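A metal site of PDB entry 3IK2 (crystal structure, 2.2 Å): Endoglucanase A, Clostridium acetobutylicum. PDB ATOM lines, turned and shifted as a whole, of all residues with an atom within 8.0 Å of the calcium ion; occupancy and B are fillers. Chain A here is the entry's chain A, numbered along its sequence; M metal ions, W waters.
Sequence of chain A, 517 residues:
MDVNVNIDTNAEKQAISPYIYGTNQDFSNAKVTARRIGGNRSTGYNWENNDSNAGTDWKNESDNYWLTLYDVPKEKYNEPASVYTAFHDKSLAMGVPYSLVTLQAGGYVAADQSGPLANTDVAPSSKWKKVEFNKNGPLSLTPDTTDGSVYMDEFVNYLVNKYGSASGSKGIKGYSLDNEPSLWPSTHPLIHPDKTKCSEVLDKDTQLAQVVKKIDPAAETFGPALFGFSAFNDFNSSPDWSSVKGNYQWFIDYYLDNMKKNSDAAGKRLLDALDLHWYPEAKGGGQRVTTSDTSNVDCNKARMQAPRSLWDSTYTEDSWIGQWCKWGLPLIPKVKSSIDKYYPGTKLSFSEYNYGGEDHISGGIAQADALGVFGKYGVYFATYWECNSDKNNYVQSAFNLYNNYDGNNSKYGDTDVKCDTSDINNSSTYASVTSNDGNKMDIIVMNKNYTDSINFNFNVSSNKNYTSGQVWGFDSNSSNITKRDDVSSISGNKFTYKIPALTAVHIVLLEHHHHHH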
ATOM      1  N   ASN A  46       5.697  -5.264 -19.073  1.00  0.00           N
ATOM      2  CA  ASN A  46       5.998  -4.501 -17.894  1.00  0.00           C
ATOM      3  C   ASN A  46       4.690  -4.141 -17.200  1.00  0.00           C
ATOM      4  O   ASN A  46       3.907  -3.379 -17.755  1.00  0.00           O
ATOM      5  CB  ASN A  46       6.733  -3.240 -18.341  1.00  0.00           C
ATOM      6  CG  ASN A  46       7.179  -2.366 -17.184  1.00  0.00           C
ATOM      7  OD1 ASN A  46       6.579  -2.366 -16.108  1.00  0.00           O
ATOM      8  ND2 ASN A  46       8.261  -1.613 -17.403  1.00  0.00           N
ATOM      9  N   TRP A  47       4.461  -4.682 -15.977  1.00  0.00           N
ATOM     10  CA  TRP A  47       3.157  -4.534 -15.310  1.00  0.00           C
ATOM     11  C   TRP A  47       2.935  -3.136 -14.757  1.00  0.00           C
ATOM     12  O   TRP A  47       1.782  -2.686 -14.570  1.00  0.00           O
ATOM     13  CB  TRP A  47       2.947  -5.616 -14.233  1.00  0.00           C
ATOM     14  CG  TRP A  47       3.648  -5.380 -12.909  1.00  0.00           C
ATOM     15  CD1 TRP A  47       4.976  -5.629 -12.595  1.00  0.00           C
ATOM     16  CD2 TRP A  47       3.069  -4.815 -11.733  1.00  0.00           C
ATOM     17  NE1 TRP A  47       5.222  -5.290 -11.284  1.00  0.00           N
ATOM     18  CE2 TRP A  47       4.072  -4.772 -10.743  1.00  0.00           C
ATOM     19  CE3 TRP A  47       1.781  -4.374 -11.409  1.00  0.00           C
ATOM     20  CZ2 TRP A  47       3.824  -4.294  -9.455  1.00  0.00           C
ATOM     21  CZ3 TRP A  47       1.535  -3.889 -10.137  1.00  0.00           C
ATOM     22  CH2 TRP A  47       2.543  -3.857  -9.176  1.00  0.00           C
ATOM     23  N   GLU A  48       4.045  -2.459 -14.481  1.00  0.00           N
ATOM     24  CA  GLU A  48       4.028  -1.085 -13.971  1.00  0.00           C
ATOM     25  C   GLU A  48       3.491  -0.064 -14.969  1.00  0.00           C
ATOM     26  O   GLU A  48       2.800   0.868 -14.573  1.00  0.00           O
ATOM     27  CB  GLU A  48       5.431  -0.695 -13.504  1.00  0.00           C
ATOM     28  CG  GLU A  48       5.993  -1.636 -12.404  1.00  0.00           C
ATOM     29  CD  GLU A  48       7.328  -1.171 -11.904  1.00  0.00           C
ATOM     30  OE1 GLU A  48       7.914  -0.270 -12.577  1.00  0.00           O
ATOM     31  OE2 GLU A  48       7.760  -1.654 -10.810  1.00  0.00           O
ATOM     32  N   LYS A 129      13.707  -2.559 -18.149  1.00  0.00           N
ATOM     33  CA  LYS A 129      13.703  -2.691 -16.697  1.00  0.00           C
ATOM     34  C   LYS A 129      14.050  -4.131 -16.334  1.00  0.00           C
ATOM     35  O   LYS A 129      13.623  -5.064 -17.003  1.00  0.00           O
ATOM     36  CB  LYS A 129      12.330  -2.321 -16.132  1.00  0.00           C
ATOM     37  CG  LYS A 129      11.874  -0.886 -16.433  1.00  0.00           C
ATOM     38  CD  LYS A 129      12.749   0.205 -15.749  1.00  0.00           C
ATOM     39  CE  LYS A 129      12.269   1.620 -16.127  1.00  0.00           C
ATOM     40  NZ  LYS A 129      13.067   2.763 -15.511  1.00  0.00           N
ATOM     41  N   LYS A 130      14.867  -4.297 -15.308  1.00  0.00           N
ATOM     42  CA  LYS A 130      15.211  -5.616 -14.766  1.00  0.00           C
ATOM     43  C   LYS A 130      14.042  -6.262 -14.020  1.00  0.00           C
ATOM     44  O   LYS A 130      13.474  -5.636 -13.110  1.00  0.00           O
ATOM     45  CB  LYS A 130      16.317  -5.439 -13.719  1.00  0.00           C
ATOM     46  CG  LYS A 130      17.682  -5.933 -14.032  1.00  0.00           C
ATOM     47  CD  LYS A 130      17.705  -7.439 -14.209  1.00  0.00           C
ATOM     48  CE  LYS A 130      19.025  -8.072 -13.725  1.00  0.00           C
ATOM     49  NZ  LYS A 130      18.740  -8.967 -12.569  1.00  0.00           N
ATOM     50  N   LYS A 135      10.778  -8.637  -3.945  1.00  0.00           N
ATOM     51  CA  LYS A 135      11.092  -7.225  -3.677  1.00  0.00           C
ATOM     52  C   LYS A 135      11.961  -7.081  -2.457  1.00  0.00           C
ATOM     53  O   LYS A 135      12.809  -6.189  -2.410  1.00  0.00           O
ATOM     54  CB  LYS A 135       9.822  -6.375  -3.537  1.00  0.00           C
ATOM     55  CG  LYS A 135      10.065  -4.877  -3.748  1.00  0.00           C
ATOM     56  CD  LYS A 135       8.798  -4.075  -3.469  1.00  0.00           C
ATOM     57  CE  LYS A 135       9.043  -2.572  -3.556  1.00  0.00           C
ATOM     58  NZ  LYS A 135       7.788  -1.761  -3.411  1.00  0.00           N
ATOM     59  N   PRO A 143       3.408   0.697  -7.670  1.00  0.00           N
ATOM     60  CA  PRO A 143       4.824   0.453  -7.816  1.00  0.00           C
ATOM     61  C   PRO A 143       5.541   1.653  -8.445  1.00  0.00           C
ATOM     62  O   PRO A 143       4.930   2.405  -9.227  1.00  0.00           O
ATOM     63  CB  PRO A 143       4.861  -0.729  -8.800  1.00  0.00           C
ATOM     64  CG  PRO A 143       3.612  -0.586  -9.571  1.00  0.00           C
ATOM     65  CD  PRO A 143       2.628  -0.202  -8.522  1.00  0.00           C
ATOM     66  N   ASP A 144       6.823   1.788  -8.128  1.00  0.00           N
ATOM     67  CA  ASP A 144       7.682   2.866  -8.643  1.00  0.00           C
ATOM     68  C   ASP A 144       8.108   2.613 -10.088  1.00  0.00           C
ATOM     69  O   ASP A 144       8.880   1.707 -10.400  1.00  0.00           O
ATOM     70  CB  ASP A 144       8.921   2.995  -7.725  1.00  0.00           C
ATOM     71  CG  ASP A 144       9.814   4.158  -8.109  1.00  0.00           C
ATOM     72  OD1 ASP A 144       9.450   4.913  -9.004  1.00  0.00           O
ATOM     73  OD2 ASP A 144      10.866   4.312  -7.475  1.00  0.00           O
ATOM     74  N   THR A 145       7.629   3.459 -10.972  1.00  0.00           N
ATOM     75  CA  THR A 145       7.918   3.337 -12.398  1.00  0.00           C
ATOM     76  C   THR A 145       9.229   4.049 -12.784  1.00  0.00           C
ATOM     77  O   THR A 145       9.685   3.979 -13.941  1.00  0.00           O
ATOM     78  CB  THR A 145       6.742   3.928 -13.180  1.00  0.00           C
ATOM     79  OG1 THR A 145       6.503   5.283 -12.738  1.00  0.00           O
ATOM     80  CG2 THR A 145       5.485   3.086 -12.910  1.00  0.00           C
ATOM     81  N   THR A 146       9.853   4.686 -11.805  1.00  0.00           N
ATOM     82  CA  THR A 146      11.006   5.536 -12.046  1.00  0.00           C
ATOM     83  C   THR A 146      12.354   4.821 -11.789  1.00  0.00           C
ATOM     84  O   THR A 146      13.396   5.276 -12.245  1.00  0.00           O
ATOM     85  CB  THR A 146      10.900   6.902 -11.281  1.00  0.00           C
ATOM     86  OG1 THR A 146      10.953   6.688  -9.867  1.00  0.00           O
ATOM     87  CG2 THR A 146       9.592   7.621 -11.606  1.00  0.00           C
ATOM     88  N   ASP A 147      12.340   3.691 -11.085  1.00  0.00           N
ATOM     89  CA  ASP A 147      13.590   2.943 -10.848  1.00  0.00           C
ATOM     90  C   ASP A 147      13.831   1.917 -11.983  1.00  0.00           C
ATOM     91  O   ASP A 147      13.055   1.890 -12.951  1.00  0.00           O
ATOM     92  CB  ASP A 147      13.590   2.310  -9.431  1.00  0.00           C
ATOM     93  CG  ASP A 147      12.524   1.247  -9.259  1.00  0.00           C
ATOM     94  OD1 ASP A 147      11.873   0.876 -10.257  1.00  0.00           O
ATOM     95  OD2 ASP A 147      12.323   0.754  -8.125  1.00  0.00           O
ATOM     96  N   GLY A 148      14.852   1.061 -11.846  1.00  0.00           N
ATOM     97  CA  GLY A 148      15.292   0.220 -12.948  1.00  0.00           C
ATOM     98  C   GLY A 148      14.786  -1.230 -12.936  1.00  0.00           C
ATOM     99  O   GLY A 148      15.249  -2.070 -13.722  1.00  0.00           O
ATOM    100  N   SER A 149      13.828  -1.500 -12.054  1.00  0.00           N
ATOM    101  CA  SER A 149      13.407  -2.853 -11.743  1.00  0.00           C
ATOM    102  C   SER A 149      11.909  -2.990 -11.667  1.00  0.00           C
ATOM    103  O   SER A 149      11.208  -2.026 -11.413  1.00  0.00           O
ATOM    104  CB  SER A 149      13.987  -3.292 -10.406  1.00  0.00           C
ATOM    105  OG  SER A 149      15.372  -3.518 -10.531  1.00  0.00           O
ATOM    106  N   VAL A 150      11.437  -4.211 -11.863  1.00  0.00           N
ATOM    107  CA  VAL A 150      10.023  -4.568 -11.757  1.00  0.00           C
ATOM    108  C   VAL A 150      10.013  -5.871 -10.929  1.00  0.00           C
ATOM    109  O   VAL A 150      10.903  -6.713 -11.116  1.00  0.00           O
ATOM    110  CB  VAL A 150       9.460  -4.788 -13.177  1.00  0.00           C
ATOM    111  CG1 VAL A 150       8.260  -5.642 -13.144  1.00  0.00           C
ATOM    112  CG2 VAL A 150       9.175  -3.439 -13.943  1.00  0.00           C
ATOM    113  N   TYR A 151       9.057  -6.007 -10.015  1.00  0.00           N
ATOM    114  CA  TYR A 151       9.009  -7.125  -9.045  1.00  0.00           C
ATOM    115  C   TYR A 151       7.781  -8.011  -9.254  1.00  0.00           C
ATOM    116  O   TYR A 151       6.655  -7.514  -9.213  1.00  0.00           O
ATOM    117  CB  TYR A 151       9.032  -6.584  -7.586  1.00  0.00           C
ATOM    118  CG  TYR A 151      10.291  -5.789  -7.347  1.00  0.00           C
ATOM    119  CD1 TYR A 151      11.468  -6.435  -6.894  1.00  0.00           C
ATOM    120  CD2 TYR A 151      10.362  -4.429  -7.655  1.00  0.00           C
ATOM    121  CE1 TYR A 151      12.652  -5.729  -6.719  1.00  0.00           C
ATOM    122  CE2 TYR A 151      11.538  -3.706  -7.487  1.00  0.00           C
ATOM    123  CZ  TYR A 151      12.680  -4.363  -7.020  1.00  0.00           C
ATOM    124  OH  TYR A 151      13.842  -3.672  -6.856  1.00  0.00           O
ATOM    125  N   GLU A 154       5.277  -8.280  -6.181  1.00  0.00           N
ATOM    126  CA  GLU A 154       4.496  -7.067  -6.064  1.00  0.00           C
ATOM    127  C   GLU A 154       3.320  -7.081  -7.067  1.00  0.00           C
ATOM    128  O   GLU A 154       2.216  -6.622  -6.746  1.00  0.00           O
ATOM    129  CB  GLU A 154       5.416  -5.857  -6.282  1.00  0.00           C
ATOM    130  CG  GLU A 154       4.753  -4.546  -6.012  1.00  0.00           C
ATOM    131  CD  GLU A 154       5.739  -3.414  -5.869  1.00  0.00           C
ATOM    132  OE1 GLU A 154       6.452  -3.126  -6.845  1.00  0.00           O
ATOM    133  OE2 GLU A 154       5.807  -2.822  -4.768  1.00  0.00           O
HETATM  134 CA    CA M   1       9.850  -0.210 -10.912  1.00  0.00          CA
HETATM  135  O   HOH W   1       9.991  -0.830  -8.669  1.00  0.00           O
HETATM  136  O   HOH W   2      10.691   0.651 -13.002  1.00  0.00           O
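The nearest printed residue that does not touch the calcium ion is Thr 145 (4.3 Å).
N of Glu 48 sits at hydrogen-bond distance from OD1 of Asn 46. The side-chain amino group (NZ) of Lys 129 sits at hydrogen-bond distance from the backbone carbonyl oxygen (O) of Asp 147, 2.7 Å away. OD1 of Asp 144 lies within hydrogen-bond range of OG1 of Thr 146.
The calcium ion is bound by O of Asp 144. The calcium ion is bound by O of Ser 149, 2.3 Å away. The calcium ion is bound by water W1. The side-chain carboxylate (OD1) of Asp 147 is bound to the calcium ion (2.4 Å). Water W2 binds the calcium ion, at 2.4 Å. OE2 of Glu 48 binds the calcium ion (2.5 Å). OE1 of Glu 48 binds the calcium ion (2.6 Å).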
